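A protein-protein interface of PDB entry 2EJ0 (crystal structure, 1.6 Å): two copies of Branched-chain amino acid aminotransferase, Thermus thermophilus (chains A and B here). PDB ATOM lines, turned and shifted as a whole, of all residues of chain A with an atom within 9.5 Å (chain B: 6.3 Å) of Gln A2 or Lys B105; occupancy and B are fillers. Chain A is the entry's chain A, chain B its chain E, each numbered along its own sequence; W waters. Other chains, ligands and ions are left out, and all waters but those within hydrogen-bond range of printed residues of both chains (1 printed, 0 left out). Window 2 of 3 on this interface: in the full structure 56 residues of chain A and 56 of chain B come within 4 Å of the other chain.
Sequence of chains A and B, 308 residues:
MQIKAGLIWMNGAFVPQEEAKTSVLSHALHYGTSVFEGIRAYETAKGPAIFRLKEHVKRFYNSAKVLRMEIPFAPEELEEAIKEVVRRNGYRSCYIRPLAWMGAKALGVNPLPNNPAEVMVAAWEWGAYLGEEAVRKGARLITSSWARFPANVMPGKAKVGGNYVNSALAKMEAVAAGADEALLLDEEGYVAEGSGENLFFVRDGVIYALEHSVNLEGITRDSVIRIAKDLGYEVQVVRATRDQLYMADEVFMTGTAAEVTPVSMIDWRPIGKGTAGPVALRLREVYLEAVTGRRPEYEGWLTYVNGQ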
ATOM      1  N   GLN A   2       1.378  -9.738  -6.757  1.00  0.00           N
ATOM      2  CA  GLN A   2       0.872 -11.136  -6.857  1.00  0.00           C
ATOM      3  C   GLN A   2      -0.631 -11.183  -6.592  1.00  0.00           C
ATOM      4  O   GLN A   2      -1.203 -10.251  -6.030  1.00  0.00           O
ATOM      5  CB  GLN A   2       1.602 -12.033  -5.852  1.00  0.00           C
ATOM      6  CG  GLN A   2       1.263 -13.512  -5.974  1.00  0.00           C
ATOM      7  CD  GLN A   2       2.016 -14.376  -4.978  1.00  0.00           C
ATOM      8  OE1 GLN A   2       3.246 -14.356  -4.925  1.00  0.00           O
ATOM      9  NE2 GLN A   2       1.278 -15.145  -4.184  1.00  0.00           N
ATOM     10  N   ILE A   3      -1.264 -12.275  -7.008  1.00  0.00           N
ATOM     11  CA  ILE A   3      -2.695 -12.453  -6.813  1.00  0.00           C
ATOM     12  C   ILE A   3      -2.935 -13.218  -5.517  1.00  0.00           C
ATOM     13  O   ILE A   3      -2.335 -14.268  -5.290  1.00  0.00           O
ATOM     14  CB  ILE A   3      -3.322 -13.242  -7.984  1.00  0.00           C
ATOM     15  CG1 ILE A   3      -3.078 -12.497  -9.300  1.00  0.00           C
ATOM     16  CG2 ILE A   3      -4.813 -13.436  -7.746  1.00  0.00           C
ATOM     17  CD1 ILE A   3      -3.562 -13.247 -10.530  1.00  0.00           C
ATOM     18  N   LYS A   4      -3.805 -12.686  -4.666  1.00  0.00           N
ATOM     19  CA  LYS A   4      -4.116 -13.330  -3.396  1.00  0.00           C
ATOM     20  C   LYS A   4      -5.322 -14.244  -3.585  1.00  0.00           C
ATOM     21  O   LYS A   4      -6.440 -13.905  -3.201  1.00  0.00           O
ATOM     22  CB  LYS A   4      -4.410 -12.267  -2.335  1.00  0.00           C
ATOM     23  CG  LYS A   4      -3.298 -11.234  -2.190  1.00  0.00           C
ATOM     24  CD  LYS A   4      -3.625 -10.185  -1.136  1.00  0.00           C
ATOM     25  CE  LYS A   4      -3.678 -10.794   0.256  1.00  0.00           C
ATOM     26  NZ  LYS A   4      -2.375 -11.410   0.635  1.00  0.00           N
ATOM     27  N   ALA A   5      -5.081 -15.408  -4.181  1.00  0.00           N
ATOM     28  CA  ALA A   5      -6.141 -16.371  -4.455  1.00  0.00           C
ATOM     29  C   ALA A   5      -6.401 -17.340  -3.309  1.00  0.00           C
ATOM     30  O   ALA A   5      -7.547 -17.689  -3.035  1.00  0.00           O
ATOM     31  CB  ALA A   5      -5.812 -17.152  -5.725  1.00  0.00           C
ATOM     32  N   GLY A   6      -5.335 -17.781  -2.651  1.00  0.00           N
ATOM     33  CA  GLY A   6      -5.490 -18.716  -1.551  1.00  0.00           C
ATOM     34  C   GLY A   6      -5.660 -20.139  -2.045  1.00  0.00           C
ATOM     35  O   GLY A   6      -4.895 -20.606  -2.891  1.00  0.00           O
ATOM     36  N   ILE A   8      -6.885 -23.068  -4.182  1.00  0.00           N
ATOM     37  CA  ILE A   8      -7.333 -23.232  -5.559  1.00  0.00           C
ATOM     38  C   ILE A   8      -7.755 -24.671  -5.845  1.00  0.00           C
ATOM     39  O   ILE A   8      -7.066 -25.620  -5.473  1.00  0.00           O
ATOM     40  CB  ILE A   8      -6.215 -22.828  -6.552  1.00  0.00           C
ATOM     41  CG1 ILE A   8      -5.916 -21.334  -6.412  1.00  0.00           C
ATOM     42  CG2 ILE A   8      -6.629 -23.167  -7.983  1.00  0.00           C
ATOM     43  CD1 ILE A   8      -4.815 -20.828  -7.318  1.00  0.00           C
ATOM     44  N   PRO A  16      -2.940 -25.408  -1.965  1.00  0.00           N
ATOM     45  CA  PRO A  16      -2.456 -24.047  -1.727  1.00  0.00           C
ATOM     46  C   PRO A  16      -2.079 -23.410  -3.064  1.00  0.00           C
ATOM     47  O   PRO A  16      -1.649 -24.104  -3.987  1.00  0.00           O
ATOM     48  CB  PRO A  16      -1.246 -24.268  -0.826  1.00  0.00           C
ATOM     49  CG  PRO A  16      -1.627 -25.500  -0.061  1.00  0.00           C
ATOM     50  CD  PRO A  16      -2.199 -26.380  -1.141  1.00  0.00           C
ATOM     51  N   GLN A  17      -2.241 -22.096  -3.164  1.00  0.00           N
ATOM     52  CA  GLN A  17      -1.929 -21.374  -4.393  1.00  0.00           C
ATOM     53  C   GLN A  17      -0.565 -21.764  -4.961  1.00  0.00           C
ATOM     54  O   GLN A  17      -0.428 -22.027  -6.155  1.00  0.00           O
ATOM     55  CB  GLN A  17      -1.961 -19.871  -4.128  1.00  0.00           C
ATOM     56  CG  GLN A  17      -1.971 -19.016  -5.379  1.00  0.00           C
ATOM     57  CD  GLN A  17      -2.042 -17.540  -5.056  1.00  0.00           C
ATOM     58  OE1 GLN A  17      -2.754 -17.131  -4.139  1.00  0.00           O
ATOM     59  NE2 GLN A  17      -1.315 -16.729  -5.815  1.00  0.00           N
ATOM     60  N   GLU A  18       0.440 -21.794  -4.095  1.00  0.00           N
ATOM     61  CA  GLU A  18       1.799 -22.144  -4.495  1.00  0.00           C
ATOM     62  C   GLU A  18       1.907 -23.516  -5.163  1.00  0.00           C
ATOM     63  O   GLU A  18       2.865 -23.780  -5.889  1.00  0.00           O
ATOM     64  CB  GLU A  18       2.728 -22.079  -3.277  1.00  0.00           C
ATOM     65  CG  GLU A  18       2.017 -22.304  -1.947  1.00  0.00           C
ATOM     66  CD  GLU A  18       1.129 -21.133  -1.550  1.00  0.00           C
ATOM     67  OE1 GLU A  18       0.254 -21.317  -0.681  1.00  0.00           O
ATOM     68  OE2 GLU A  18       1.311 -20.026  -2.101  1.00  0.00           O
ATOM     69  N   GLU A  19       0.931 -24.384  -4.925  1.00  0.00           N
ATOM     70  CA  GLU A  19       0.946 -25.718  -5.519  1.00  0.00           C
ATOM     71  C   GLU A  19       0.127 -25.802  -6.804  1.00  0.00           C
ATOM     72  O   GLU A  19       0.157 -26.818  -7.499  1.00  0.00           O
ATOM     73  CB  GLU A  19       0.422 -26.754  -4.522  1.00  0.00           C
ATOM     74  CG  GLU A  19       1.252 -26.876  -3.256  1.00  0.00           C
ATOM     75  CD  GLU A  19       0.770 -27.992  -2.349  1.00  0.00           C
ATOM     76  OE1 GLU A  19       1.316 -28.123  -1.233  1.00  0.00           O
ATOM     77  OE2 GLU A  19      -0.149 -28.738  -2.751  1.00  0.00           O
ATOM     78  N   TRP A 124     -10.603 -14.514  -5.875  1.00  0.00           N
ATOM     79  CA  TRP A 124      -9.926 -13.516  -5.062  1.00  0.00           C
ATOM     80  C   TRP A 124     -10.890 -12.403  -4.688  1.00  0.00           C
ATOM     81  O   TRP A 124     -11.838 -12.116  -5.422  1.00  0.00           O
ATOM     82  CB  TRP A 124      -8.707 -12.955  -5.801  1.00  0.00           C
ATOM     83  CG  TRP A 124      -8.971 -12.504  -7.206  1.00  0.00           C
ATOM     84  CD1 TRP A 124      -9.456 -11.291  -7.605  1.00  0.00           C
ATOM     85  CD2 TRP A 124      -8.746 -13.260  -8.401  1.00  0.00           C
ATOM     86  NE1 TRP A 124      -9.541 -11.243  -8.979  1.00  0.00           N
ATOM     87  CE2 TRP A 124      -9.111 -12.439  -9.491  1.00  0.00           C
ATOM     88  CE3 TRP A 124      -8.269 -14.553  -8.656  1.00  0.00           C
ATOM     89  CZ2 TRP A 124      -9.012 -12.870 -10.821  1.00  0.00           C
ATOM     90  CZ3 TRP A 124      -8.173 -14.983  -9.981  1.00  0.00           C
ATOM     91  CH2 TRP A 124      -8.543 -14.141 -11.044  1.00  0.00           C
ATOM     92  N   LEU B  25      -2.248 -19.313 -12.726  1.00  0.00           N
ATOM     93  CA  LEU B  25      -2.791 -17.960 -12.766  1.00  0.00           C
ATOM     94  C   LEU B  25      -1.964 -17.110 -13.724  1.00  0.00           C
ATOM     95  O   LEU B  25      -2.126 -15.889 -13.792  1.00  0.00           O
ATOM     96  CB  LEU B  25      -2.782 -17.328 -11.370  1.00  0.00           C
ATOM     97  CG  LEU B  25      -3.675 -17.999 -10.326  1.00  0.00           C
ATOM     98  CD1 LEU B  25      -3.564 -17.244  -9.011  1.00  0.00           C
ATOM     99  CD2 LEU B  25      -5.118 -18.020 -10.807  1.00  0.00           C
ATOM    100  N   SER B  26      -1.068 -17.760 -14.462  1.00  0.00           N
ATOM    101  CA  SER B  26      -0.230 -17.057 -15.428  1.00  0.00           C
ATOM    102  C   SER B  26      -1.087 -16.423 -16.519  1.00  0.00           C
ATOM    103  O   SER B  26      -1.950 -17.077 -17.104  1.00  0.00           O
ATOM    104  CB  SER B  26       0.776 -18.015 -16.066  1.00  0.00           C
ATOM    105  OG  SER B  26       1.777 -18.386 -15.136  1.00  0.00           O
ATOM    106  N   HIS B  27      -0.831 -15.147 -16.784  1.00  0.00           N
ATOM    107  CA  HIS B  27      -1.564 -14.379 -17.787  1.00  0.00           C
ATOM    108  C   HIS B  27      -1.675 -15.130 -19.120  1.00  0.00           C
ATOM    109  O   HIS B  27      -2.753 -15.207 -19.716  1.00  0.00           O
ATOM    110  CB  HIS B  27      -0.857 -13.031 -17.978  1.00  0.00           C
ATOM    111  CG  HIS B  27      -1.696 -11.974 -18.631  1.00  0.00           C
ATOM    112  ND1 HIS B  27      -1.805 -11.846 -20.000  1.00  0.00           N
ATOM    113  CD2 HIS B  27      -2.423 -10.961 -18.101  1.00  0.00           C
ATOM    114  CE1 HIS B  27      -2.560 -10.798 -20.284  1.00  0.00           C
ATOM    115  NE2 HIS B  27      -2.948 -10.243 -19.148  1.00  0.00           N
ATOM    116  N   GLY B 103       3.505 -13.849 -16.907  1.00  0.00           N
ATOM    117  CA  GLY B 103       3.243 -14.552 -15.662  1.00  0.00           C
ATOM    118  C   GLY B 103       1.991 -14.229 -14.868  1.00  0.00           C
ATOM    119  O   GLY B 103       1.046 -13.625 -15.374  1.00  0.00           O
ATOM    120  N   ALA B 104       2.011 -14.615 -13.594  1.00  0.00           N
ATOM    121  CA  ALA B 104       0.864 -14.442 -12.705  1.00  0.00           C
ATOM    122  C   ALA B 104       0.837 -13.239 -11.768  1.00  0.00           C
ATOM    123  O   ALA B 104       0.268 -13.327 -10.678  1.00  0.00           O
ATOM    124  CB  ALA B 104       0.673 -15.716 -11.890  1.00  0.00           C
ATOM    125  N   LYS B 105       1.430 -12.121 -12.168  1.00  0.00           N
ATOM    126  CA  LYS B 105       1.410 -10.941 -11.311  1.00  0.00           C
ATOM    127  C   LYS B 105      -0.006 -10.386 -11.197  1.00  0.00           C
ATOM    128  O   LYS B 105      -0.406  -9.891 -10.142  1.00  0.00           O
ATOM    129  CB  LYS B 105       2.340  -9.856 -11.858  1.00  0.00           C
ATOM    130  CG  LYS B 105       3.818 -10.167 -11.691  1.00  0.00           C
ATOM    131  CD  LYS B 105       4.675  -9.025 -12.209  1.00  0.00           C
ATOM    132  CE  LYS B 105       6.152  -9.297 -11.991  1.00  0.00           C
ATOM    133  NZ  LYS B 105       6.994  -8.169 -12.476  1.00  0.00           N
ATOM    134  N   ALA B 106      -0.762 -10.478 -12.287  1.00  0.00           N
ATOM    135  CA  ALA B 106      -2.136  -9.981 -12.316  1.00  0.00           C
ATOM    136  C   ALA B 106      -2.896 -10.615 -13.474  1.00  0.00           C
ATOM    137  O   ALA B 106      -2.289 -11.164 -14.396  1.00  0.00           O
ATOM    138  CB  ALA B 106      -2.135  -8.465 -12.461  1.00  0.00           C
ATOM    139  N   LEU B 107      -4.223 -10.546 -13.426  1.00  0.00           N
ATOM    140  CA  LEU B 107      -5.031 -11.123 -14.494  1.00  0.00           C
ATOM    141  C   LEU B 107      -5.931 -10.142 -15.238  1.00  0.00           C
ATOM    142  O   LEU B 107      -6.986 -10.515 -15.751  1.00  0.00           O
ATOM    143  CB  LEU B 107      -5.844 -12.315 -13.975  1.00  0.00           C
ATOM    144  CG  LEU B 107      -5.025 -13.612 -13.891  1.00  0.00           C
ATOM    145  CD1 LEU B 107      -5.866 -14.732 -13.306  1.00  0.00           C
ATOM    146  CD2 LEU B 107      -4.534 -13.997 -15.288  1.00  0.00           C
ATOM    147  N   PRO B 113       1.313  -4.831 -16.934  1.00  0.00           N
ATOM    148  CA  PRO B 113       1.644  -4.941 -15.509  1.00  0.00           C
ATOM    149  C   PRO B 113       2.379  -6.236 -15.156  1.00  0.00           C
ATOM    150  O   PRO B 113       2.979  -6.348 -14.087  1.00  0.00           O
ATOM    151  CB  PRO B 113       0.275  -4.870 -14.832  1.00  0.00           C
ATOM    152  CG  PRO B 113      -0.517  -4.016 -15.766  1.00  0.00           C
ATOM    153  CD  PRO B 113      -0.125  -4.566 -17.117  1.00  0.00           C
ATOM    154  N   ASN B 114       2.332  -7.211 -16.060  1.00  0.00           N
ATOM    155  CA  ASN B 114       2.962  -8.505 -15.823  1.00  0.00           C
ATOM    156  C   ASN B 114       4.424  -8.611 -16.248  1.00  0.00           C
ATOM    157  O   ASN B 114       5.089  -9.600 -15.936  1.00  0.00           O
ATOM    158  CB  ASN B 114       2.153  -9.609 -16.511  1.00  0.00           C
ATOM    159  CG  ASN B 114       0.730  -9.697 -15.994  1.00  0.00           C
ATOM    160  OD1 ASN B 114      -0.036  -8.739 -16.088  1.00  0.00           O
ATOM    161  ND2 ASN B 114       0.370 -10.848 -15.442  1.00  0.00           N
ATOM    162  N   ASN B 115       4.925  -7.606 -16.960  1.00  0.00           N
ATOM    163  CA  ASN B 115       6.317  -7.618 -17.399  1.00  0.00           C
ATOM    164  C   ASN B 115       7.261  -7.618 -16.201  1.00  0.00           C
ATOM    165  O   ASN B 115       6.918  -7.108 -15.136  1.00  0.00           O
ATOM    166  CB  ASN B 115       6.618  -6.405 -18.283  1.00  0.00           C
ATOM    167  CG  ASN B 115       6.337  -6.671 -19.749  1.00  0.00           C
ATOM    168  OD1 ASN B 115       6.769  -7.686 -20.293  1.00  0.00           O
ATOM    169  ND2 ASN B 115       5.626  -5.754 -20.399  1.00  0.00           N
ATOM    170  N   PRO B 116       8.463  -8.197 -16.360  1.00  0.00           N
ATOM    171  CA  PRO B 116       8.955  -8.837 -17.584  1.00  0.00           C
ATOM    172  C   PRO B 116       8.403 -10.248 -17.751  1.00  0.00           C
ATOM    173  O   PRO B 116       7.929 -10.863 -16.795  1.00  0.00           O
ATOM    174  CB  PRO B 116      10.465  -8.832 -17.385  1.00  0.00           C
ATOM    175  CG  PRO B 116      10.582  -9.079 -15.920  1.00  0.00           C
ATOM    176  CD  PRO B 116       9.525  -8.154 -15.338  1.00  0.00           C
HETATM  177  O   HOH W   1       0.030 -14.536  -8.447  1.00  0.00           O
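Among the printed residues, merely in contact across the chains: Trp A124 with Leu B107 (3.6 Å), Ile A3 with Leu B107 (3.7 Å), Ile A3 with Ala B104 (3.7 Å), Gln A2 with Lys B105 (3.7 Å), Ile A3 with Lys B105 (3.8 Å), Gln A17 with Leu B25 (3.9 Å), Ala A5 with Leu B25 (3.98 Å) and Ile A3 with Ala B106 (3.99 Å).
O of Ile A3 is in hydrogen-bond range of NE2 of Gln A17 (2.7 Å). OE1 of Gln A17 is in hydrogen-bond range of N of Gly A6 (3.0 Å). OE1 of Gln A17 is in hydrogen-bond range of N of Ala A5 (2.9 Å). NE2 of Gln A2 sits close to NE2 of Gln A17 (3.4 Å). The backbone carbonyl oxygen of Ala B106 lies within hydrogen-bond range of the side-chain amide nitrogen of Asn B114, 2.9 Å away. The side-chain amino group of Lys B105 sits at hydrogen-bond distance from the backbone carbonyl oxygen of Asn B115.
Printed residues of chain B that touch a printed residue of chain A: Leu B25, Ala B104, Lys B105, Ala B106 and Leu B107. Among the printed residues, 8 pairs touch across the chains. Among the printed residues, no Asp or Glu carboxylate lies within 4 Å of a Lys or Arg side-chain nitrogen of the other chain.
Gln A2 touches one residue of chain B. Lys A4 touches none of the printed residues of chain B. Of the printed residues of chain B, Ala A5 touches Leu B25. Gly A6 touches none of the printed residues of chain B. Of the printed residues of chain B, Gln A17 touches Leu B25 (3.9 Å). Printed residues of chain A within 4 Å of Leu B25: Ala A5 and Gln A17. Of the printed residues of chain A, Leu B107 touches Ile A3 (3.7 Å) and Trp A124 (3.6 Å). No residue of chain A comes within 4 Å of Asn B114.
No position is printed for both chains. Of the 8 pairs that touch across the chains among the printed residues, none has its exchanged pair printed and touching as well.
Water W1 lies within hydrogen-bond range of O of Ala B104 and N of Ile A3.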
